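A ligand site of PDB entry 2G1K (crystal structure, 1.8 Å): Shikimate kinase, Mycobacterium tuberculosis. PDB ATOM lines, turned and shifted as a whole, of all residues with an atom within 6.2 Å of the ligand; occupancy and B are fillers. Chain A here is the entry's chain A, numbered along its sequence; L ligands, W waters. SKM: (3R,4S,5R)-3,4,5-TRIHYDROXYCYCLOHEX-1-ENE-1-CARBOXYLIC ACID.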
ATOM      1  N   PRO A  11      24.953  21.106  -2.223  1.00  0.00           N
ATOM      2  CA  PRO A  11      25.435  22.012  -3.264  1.00  0.00           C
ATOM      3  C   PRO A  11      25.857  23.270  -2.499  1.00  0.00           C
ATOM      4  O   PRO A  11      25.201  23.662  -1.530  1.00  0.00           O
ATOM      5  CB  PRO A  11      24.192  22.245  -4.115  1.00  0.00           C
ATOM      6  CG  PRO A  11      23.059  22.006  -3.171  1.00  0.00           C
ATOM      7  CD  PRO A  11      23.530  20.788  -2.410  1.00  0.00           C
ATOM      8  N   LYS A  15      32.342  21.394  -3.190  1.00  0.00           N
ATOM      9  CA  LYS A  15      32.876  20.190  -3.811  1.00  0.00           C
ATOM     10  C   LYS A  15      33.693  20.496  -5.068  1.00  0.00           C
ATOM     11  O   LYS A  15      34.806  19.994  -5.215  1.00  0.00           O
ATOM     12  CB  LYS A  15      31.746  19.206  -4.129  1.00  0.00           C
ATOM     13  CG  LYS A  15      30.964  18.741  -2.909  1.00  0.00           C
ATOM     14  CD  LYS A  15      29.954  17.657  -3.248  1.00  0.00           C
ATOM     15  CE  LYS A  15      28.899  18.166  -4.222  1.00  0.00           C
ATOM     16  NZ  LYS A  15      28.086  19.251  -3.636  1.00  0.00           N
ATOM     17  N   ASP A  32      33.446  14.682 -11.645  1.00  0.00           N
ATOM     18  CA  ASP A  32      32.192  15.051 -10.992  1.00  0.00           C
ATOM     19  C   ASP A  32      31.135  14.139 -11.592  1.00  0.00           C
ATOM     20  O   ASP A  32      30.967  14.094 -12.800  1.00  0.00           O
ATOM     21  CB  ASP A  32      31.869  16.529 -11.274  1.00  0.00           C
ATOM     22  CG  ASP A  32      30.493  16.936 -10.754  1.00  0.00           C
ATOM     23  OD1 ASP A  32      29.950  16.243  -9.864  1.00  0.00           O
ATOM     24  OD2 ASP A  32      29.971  17.960 -11.235  1.00  0.00           O
ATOM     25  N   ASP A  34      28.035  14.402 -11.763  1.00  0.00           N
ATOM     26  CA  ASP A  34      26.990  15.109 -12.501  1.00  0.00           C
ATOM     27  C   ASP A  34      27.434  15.225 -13.961  1.00  0.00           C
ATOM     28  O   ASP A  34      26.637  15.012 -14.880  1.00  0.00           O
ATOM     29  CB  ASP A  34      26.756  16.513 -11.945  1.00  0.00           C
ATOM     30  CG  ASP A  34      25.876  16.529 -10.716  1.00  0.00           C
ATOM     31  OD1 ASP A  34      25.369  15.451 -10.331  1.00  0.00           O
ATOM     32  OD2 ASP A  34      25.693  17.612 -10.140  1.00  0.00           O
ATOM     33  N   ILE A  37      27.199  11.916 -15.679  1.00  0.00           N
ATOM     34  CA  ILE A  37      25.830  11.597 -16.034  1.00  0.00           C
ATOM     35  C   ILE A  37      25.444  12.298 -17.331  1.00  0.00           C
ATOM     36  O   ILE A  37      24.749  11.734 -18.182  1.00  0.00           O
ATOM     37  CB  ILE A  37      24.855  12.012 -14.920  1.00  0.00           C
ATOM     38  CG1 ILE A  37      25.023  11.080 -13.718  1.00  0.00           C
ATOM     39  CG2 ILE A  37      23.421  12.025 -15.450  1.00  0.00           C
ATOM     40  CD1 ILE A  37      24.286  11.549 -12.459  1.00  0.00           C
ATOM     41  N   ILE A  45      21.125  17.572 -16.768  1.00  0.00           N
ATOM     42  CA  ILE A  45      20.513  17.055 -15.550  1.00  0.00           C
ATOM     43  C   ILE A  45      19.104  17.610 -15.377  1.00  0.00           C
ATOM     44  O   ILE A  45      18.198  16.904 -14.924  1.00  0.00           O
ATOM     45  CB  ILE A  45      21.378  17.414 -14.318  1.00  0.00           C
ATOM     46  CG1 ILE A  45      22.726  16.680 -14.436  1.00  0.00           C
ATOM     47  CG2 ILE A  45      20.654  17.033 -13.029  1.00  0.00           C
ATOM     48  CD1 ILE A  45      23.653  16.864 -13.258  1.00  0.00           C
ATOM     49  N   PHE A  49      15.383  15.437 -14.797  1.00  0.00           N
ATOM     50  CA  PHE A  49      14.434  15.708 -13.728  1.00  0.00           C
ATOM     51  C   PHE A  49      13.071  16.141 -14.263  1.00  0.00           C
ATOM     52  O   PHE A  49      12.042  15.684 -13.790  1.00  0.00           O
ATOM     53  CB  PHE A  49      14.937  16.824 -12.814  1.00  0.00           C
ATOM     54  CG  PHE A  49      15.727  16.343 -11.635  1.00  0.00           C
ATOM     55  CD1 PHE A  49      17.077  16.047 -11.757  1.00  0.00           C
ATOM     56  CD2 PHE A  49      15.106  16.160 -10.398  1.00  0.00           C
ATOM     57  CE1 PHE A  49      17.815  15.589 -10.663  1.00  0.00           C
ATOM     58  CE2 PHE A  49      15.821  15.703  -9.296  1.00  0.00           C
ATOM     59  CZ  PHE A  49      17.177  15.407  -9.426  1.00  0.00           C
ATOM     60  N   GLU A  54      12.843  12.557 -10.697  1.00  0.00           N
ATOM     61  CA  GLU A  54      13.931  12.315  -9.756  1.00  0.00           C
ATOM     62  C   GLU A  54      14.213  10.838  -9.514  1.00  0.00           C
ATOM     63  O   GLU A  54      15.377  10.439  -9.428  1.00  0.00           O
ATOM     64  CB  GLU A  54      13.648  13.000  -8.424  1.00  0.00           C
ATOM     65  CG  GLU A  54      14.684  12.707  -7.357  1.00  0.00           C
ATOM     66  CD  GLU A  54      14.617  13.673  -6.177  1.00  0.00           C
ATOM     67  OE1 GLU A  54      13.504  14.082  -5.806  1.00  0.00           O
ATOM     68  OE2 GLU A  54      15.684  13.995  -5.615  1.00  0.00           O
ATOM     69  N   PHE A  57      16.216   9.616 -12.187  1.00  0.00           N
ATOM     70  CA  PHE A  57      17.513  10.286 -12.109  1.00  0.00           C
ATOM     71  C   PHE A  57      18.407   9.575 -11.086  1.00  0.00           C
ATOM     72  O   PHE A  57      19.598   9.356 -11.345  1.00  0.00           O
ATOM     73  CB  PHE A  57      17.395  11.750 -11.697  1.00  0.00           C
ATOM     74  CG  PHE A  57      18.723  12.401 -11.476  1.00  0.00           C
ATOM     75  CD1 PHE A  57      19.540  12.719 -12.567  1.00  0.00           C
ATOM     76  CD2 PHE A  57      19.220  12.600 -10.190  1.00  0.00           C
ATOM     77  CE1 PHE A  57      20.824  13.222 -12.378  1.00  0.00           C
ATOM     78  CE2 PHE A  57      20.516  13.103  -9.994  1.00  0.00           C
ATOM     79  CZ  PHE A  57      21.314  13.408 -11.083  1.00  0.00           C
ATOM     80  N   ARG A  58      17.828   9.231  -9.944  1.00  0.00           N
ATOM     81  CA  ARG A  58      18.609   8.563  -8.890  1.00  0.00           C
ATOM     82  C   ARG A  58      19.131   7.188  -9.314  1.00  0.00           C
ATOM     83  O   ARG A  58      20.234   6.808  -8.921  1.00  0.00           O
ATOM     84  CB  ARG A  58      17.779   8.429  -7.604  1.00  0.00           C
ATOM     85  CG  ARG A  58      17.375   9.747  -6.952  1.00  0.00           C
ATOM     86  CD  ARG A  58      18.585  10.594  -6.547  1.00  0.00           C
ATOM     87  NE  ARG A  58      18.189  11.927  -6.095  1.00  0.00           N
ATOM     88  CZ  ARG A  58      18.992  12.979  -6.073  1.00  0.00           C
ATOM     89  NH1 ARG A  58      20.255  12.865  -6.460  1.00  0.00           N
ATOM     90  NH2 ARG A  58      18.534  14.165  -5.678  1.00  0.00           N
ATOM     91  N   GLU A  61      22.044   7.906 -11.653  1.00  0.00           N
ATOM     92  CA  GLU A  61      23.151   8.424 -10.848  1.00  0.00           C
ATOM     93  C   GLU A  61      23.877   7.311 -10.091  1.00  0.00           C
ATOM     94  O   GLU A  61      25.103   7.283 -10.038  1.00  0.00           O
ATOM     95  CB  GLU A  61      22.629   9.481  -9.872  1.00  0.00           C
ATOM     96  CG  GLU A  61      23.641   9.982  -8.851  1.00  0.00           C
ATOM     97  CD  GLU A  61      23.066  11.070  -7.948  1.00  0.00           C
ATOM     98  OE1 GLU A  61      22.007  10.831  -7.316  1.00  0.00           O
ATOM     99  OE2 GLU A  61      23.660  12.170  -7.877  1.00  0.00           O
ATOM    100  N   LEU A  78      30.712  13.695  -5.679  1.00  0.00           N
ATOM    101  CA  LEU A  78      29.384  13.150  -5.931  1.00  0.00           C
ATOM    102  C   LEU A  78      28.304  14.222  -5.861  1.00  0.00           C
ATOM    103  O   LEU A  78      28.376  15.107  -5.005  1.00  0.00           O
ATOM    104  CB  LEU A  78      29.025  12.081  -4.905  1.00  0.00           C
ATOM    105  CG  LEU A  78      29.979  10.919  -4.655  1.00  0.00           C
ATOM    106  CD1 LEU A  78      29.240   9.859  -3.837  1.00  0.00           C
ATOM    107  CD2 LEU A  78      30.459  10.336  -5.970  1.00  0.00           C
ATOM    108  N   GLY A  79      27.313  14.121  -6.738  1.00  0.00           N
ATOM    109  CA  GLY A  79      26.207  15.072  -6.725  1.00  0.00           C
ATOM    110  C   GLY A  79      25.644  15.110  -5.320  1.00  0.00           C
ATOM    111  O   GLY A  79      25.633  14.089  -4.618  1.00  0.00           O
ATOM    112  N   GLY A  80      25.167  16.276  -4.912  1.00  0.00           N
ATOM    113  CA  GLY A  80      24.629  16.460  -3.572  1.00  0.00           C
ATOM    114  C   GLY A  80      23.637  15.448  -3.060  1.00  0.00           C
ATOM    115  O   GLY A  80      23.628  15.150  -1.863  1.00  0.00           O
ATOM    116  N   GLY A  81      22.804  14.906  -3.932  1.00  0.00           N
ATOM    117  CA  GLY A  81      21.814  13.942  -3.482  1.00  0.00           C
ATOM    118  C   GLY A  81      22.133  12.472  -3.687  1.00  0.00           C
ATOM    119  O   GLY A  81      21.289  11.615  -3.435  1.00  0.00           O
ATOM    120  N   ALA A  82      23.336  12.161  -4.148  1.00  0.00           N
ATOM    121  CA  ALA A  82      23.694  10.773  -4.380  1.00  0.00           C
ATOM    122  C   ALA A  82      23.541   9.889  -3.131  1.00  0.00           C
ATOM    123  O   ALA A  82      23.107   8.743  -3.225  1.00  0.00           O
ATOM    124  CB  ALA A  82      25.135  10.687  -4.902  1.00  0.00           C
ATOM    125  N   VAL A 116      21.133  26.179 -12.872  1.00  0.00           N
ATOM    126  CA  VAL A 116      19.850  25.485 -12.769  1.00  0.00           C
ATOM    127  C   VAL A 116      19.946  24.383 -11.725  1.00  0.00           C
ATOM    128  O   VAL A 116      20.832  23.535 -11.796  1.00  0.00           O
ATOM    129  CB  VAL A 116      19.435  24.840 -14.127  1.00  0.00           C
ATOM    130  CG1 VAL A 116      18.138  24.078 -13.957  1.00  0.00           C
ATOM    131  CG2 VAL A 116      19.285  25.924 -15.207  1.00  0.00           C
ATOM    132  N   ARG A 117      19.044  24.407 -10.740  1.00  0.00           N
ATOM    133  CA  ARG A 117      19.019  23.398  -9.662  1.00  0.00           C
ATOM    134  C   ARG A 117      17.574  22.944  -9.432  1.00  0.00           C
ATOM    135  O   ARG A 117      16.807  23.604  -8.737  1.00  0.00           O
ATOM    136  CB  ARG A 117      19.569  23.991  -8.355  1.00  0.00           C
ATOM    137  CG  ARG A 117      20.972  24.557  -8.453  1.00  0.00           C
ATOM    138  CD  ARG A 117      21.341  25.351  -7.208  1.00  0.00           C
ATOM    139  NE  ARG A 117      22.624  26.057  -7.360  1.00  0.00           N
ATOM    140  CZ  ARG A 117      23.803  25.463  -7.372  1.00  0.00           C
ATOM    141  NH1 ARG A 117      23.884  24.144  -7.240  1.00  0.00           N
ATOM    142  NH2 ARG A 117      24.901  26.180  -7.527  1.00  0.00           N
ATOM    143  N   PRO A 118      17.192  21.795 -10.008  1.00  0.00           N
ATOM    144  CA  PRO A 118      15.839  21.262  -9.868  1.00  0.00           C
ATOM    145  C   PRO A 118      15.271  21.209  -8.448  1.00  0.00           C
ATOM    146  O   PRO A 118      14.072  21.406  -8.241  1.00  0.00           O
ATOM    147  CB  PRO A 118      15.939  19.884 -10.515  1.00  0.00           C
ATOM    148  CG  PRO A 118      16.941  20.113 -11.595  1.00  0.00           C
ATOM    149  CD  PRO A 118      18.001  20.936 -10.891  1.00  0.00           C
ATOM    150  N   LEU A 119      16.149  20.937  -7.477  1.00  0.00           N
ATOM    151  CA  LEU A 119      15.705  20.832  -6.091  1.00  0.00           C
ATOM    152  C   LEU A 119      16.005  22.058  -5.224  1.00  0.00           C
ATOM    153  O   LEU A 119      15.726  22.060  -4.013  1.00  0.00           O
ATOM    154  CB  LEU A 119      16.321  19.581  -5.459  1.00  0.00           C
ATOM    155  CG  LEU A 119      15.939  18.273  -6.145  1.00  0.00           C
ATOM    156  CD1 LEU A 119      16.590  17.093  -5.434  1.00  0.00           C
ATOM    157  CD2 LEU A 119      14.437  18.114  -6.142  1.00  0.00           C
ATOM    158  N   LEU A 120      16.575  23.099  -5.830  1.00  0.00           N
ATOM    159  CA  LEU A 120      16.895  24.333  -5.119  1.00  0.00           C
ATOM    160  C   LEU A 120      16.539  25.556  -5.949  1.00  0.00           C
ATOM    161  O   LEU A 120      17.413  26.360  -6.285  1.00  0.00           O
ATOM    162  CB  LEU A 120      18.382  24.397  -4.764  1.00  0.00           C
ATOM    163  CG  LEU A 120      18.828  23.814  -3.435  1.00  0.00           C
ATOM    164  CD1 LEU A 120      20.312  24.093  -3.253  1.00  0.00           C
ATOM    165  CD2 LEU A 120      18.016  24.439  -2.309  1.00  0.00           C
ATOM    166  N   LEU A 132      16.856  20.162   2.826  1.00  0.00           N
ATOM    167  CA  LEU A 132      17.799  19.198   2.283  1.00  0.00           C
ATOM    168  C   LEU A 132      18.868  18.888   3.324  1.00  0.00           C
ATOM    169  O   LEU A 132      19.272  17.742   3.480  1.00  0.00           O
ATOM    170  CB  LEU A 132      18.480  19.738   1.014  1.00  0.00           C
ATOM    171  CG  LEU A 132      17.619  20.008  -0.223  1.00  0.00           C
ATOM    172  CD1 LEU A 132      18.481  20.613  -1.326  1.00  0.00           C
ATOM    173  CD2 LEU A 132      16.970  18.708  -0.691  1.00  0.00           C
ATOM    174  N   ARG A 136      19.561  15.153   4.720  1.00  0.00           N
ATOM    175  CA  ARG A 136      20.798  14.514   4.267  1.00  0.00           C
ATOM    176  C   ARG A 136      21.970  14.522   5.224  1.00  0.00           C
ATOM    177  O   ARG A 136      22.922  13.766   5.034  1.00  0.00           O
ATOM    178  CB  ARG A 136      21.246  15.145   2.957  1.00  0.00           C
ATOM    179  CG  ARG A 136      20.214  15.032   1.849  1.00  0.00           C
ATOM    180  CD  ARG A 136      20.690  15.791   0.632  1.00  0.00           C
ATOM    181  NE  ARG A 136      19.736  15.717  -0.463  1.00  0.00           N
ATOM    182  CZ  ARG A 136      19.925  16.317  -1.631  1.00  0.00           C
ATOM    183  NH1 ARG A 136      21.028  17.034  -1.820  1.00  0.00           N
ATOM    184  NH2 ARG A 136      19.030  16.222  -2.600  1.00  0.00           N
ATOM    185  N   TYR A 140      25.239  11.964   5.049  1.00  0.00           N
ATOM    186  CA  TYR A 140      26.622  12.357   4.769  1.00  0.00           C
ATOM    187  C   TYR A 140      27.476  11.808   5.911  1.00  0.00           C
ATOM    188  O   TYR A 140      28.536  11.236   5.685  1.00  0.00           O
ATOM    189  CB  TYR A 140      26.757  13.878   4.708  1.00  0.00           C
ATOM    190  CG  TYR A 140      26.053  14.538   3.538  1.00  0.00           C
ATOM    191  CD1 TYR A 140      26.271  14.105   2.229  1.00  0.00           C
ATOM    192  CD2 TYR A 140      25.191  15.615   3.742  1.00  0.00           C
ATOM    193  CE1 TYR A 140      25.631  14.735   1.141  1.00  0.00           C
ATOM    194  CE2 TYR A 140      24.556  16.231   2.670  1.00  0.00           C
ATOM    195  CZ  TYR A 140      24.778  15.784   1.377  1.00  0.00           C
ATOM    196  OH  TYR A 140      24.138  16.394   0.326  1.00  0.00           O
HETATM  197  O12 SKM L   1      23.009  16.018  -8.963  1.00  0.00           O
HETATM  198  C8  SKM L   1      22.570  17.377  -9.206  1.00  0.00           C
HETATM  199  C6  SKM L   1      21.027  17.411  -9.195  1.00  0.00           C
HETATM  200  O7  SKM L   1      20.599  18.762  -9.443  1.00  0.00           O
HETATM  201  C5  SKM L   1      20.440  16.960  -7.846  1.00  0.00           C
HETATM  202  C4  SKM L   1      21.243  17.458  -6.628  1.00  0.00           C
HETATM  203  C1  SKM L   1      20.660  17.282  -5.282  1.00  0.00           C
HETATM  204  O2  SKM L   1      20.883  18.068  -4.365  1.00  0.00           O
HETATM  205  O3  SKM L   1      19.857  16.239  -5.026  1.00  0.00           O
HETATM  206  C10 SKM L   1      22.466  18.041  -6.750  1.00  0.00           C
HETATM  207  C9  SKM L   1      23.161  18.253  -8.084  1.00  0.00           C
HETATM  208  O11 SKM L   1      24.546  17.941  -7.941  1.00  0.00           O
HETATM  209  O   HOH W   1      21.960  20.026 -11.486  1.00  0.00           O
HETATM  210  O   HOH W   2      24.834  20.844  -7.945  1.00  0.00           O
HETATM  211  O   HOH W   3      25.782  19.487  -5.356  1.00  0.00           O
HETATM  212  O   HOH W   4      19.064  20.497  -7.660  1.00  0.00           O
HETATM  213  O   HOH W   5      20.195  20.760  -5.071  1.00  0.00           O
HETATM  214  O   HOH W   6      22.780  14.452  -6.718  1.00  0.00           O
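NH1 of Arg 136 is in hydrogen-bond range of O of Gly 80, 3.2 Å away.
NH1 of Arg 58 sits close to O of Gly 81 (3.4 Å).
The side-chain carboxylate (OE2) of Glu 54 is in salt-bridge range of the guanidinium group (NH2) of Arg 58.
NH1 of Arg 58 lies within salt-bridge range of OE1 of Glu 61 (2.8 Å).
OH of Tyr 140 sits at hydrogen-bond distance from O of Gly 80, 2.6 Å away.
N of Asp 34 sits close to OD1 of Asp 32, 3.3 Å away.
Water W4 bridges an oxygen (O7) of the ligand (2.9 Å) and the backbone NH (N) of Leu 119 (3.0 Å).
Water W3 lies within hydrogen-bond range of NZ of Lys 15 (2.9 Å), O11 of the ligand (3.3 Å) and N of Gly 80 (3.3 Å).
The guanidinium group (NH2) of Arg 58 lies within salt-bridge range of an oxygen (O3) of the ligand (2.5 Å).
An oxygen (O3) of the ligand lies close to the backbone NH (N) of Gly 81, at 3.4 Å.
The side-chain carboxylate (OD2) of Asp 34 sits at hydrogen-bond distance from an oxygen (O11) of the ligand, 2.5 Å away.
The guanidinium group (NH2) of Arg 136 is in salt-bridge range of an oxygen (O3) of the ligand, 2.6 Å away.
Residues that only touch the ligand: Ile 45 (3.9 Å), Phe 49 (3.9 Å), Phe 57 (3.8 Å), Gly 79 (3.5 Å), Gly 80 (3.5 Å), Pro 118 (3.7 Å) and Leu 119 (3.4 Å).
Hydrophobic or aromatic side chains that line the ligand: Ile 45, Phe 49, Phe 57, Pro 118 and Leu 119.
11 residues have an atom within 4 Å of the ligand: Asp 34, Ile 45, Phe 49, Phe 57, Arg 58, Gly 79, Gly 80, Gly 81, Pro 118, Leu 119 and Arg 136.
Along chain A the residues within 4 Å of the ligand span positions 34 to 136.
The nearest printed residue that does not touch the ligand is Glu 61 (4.1 Å).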
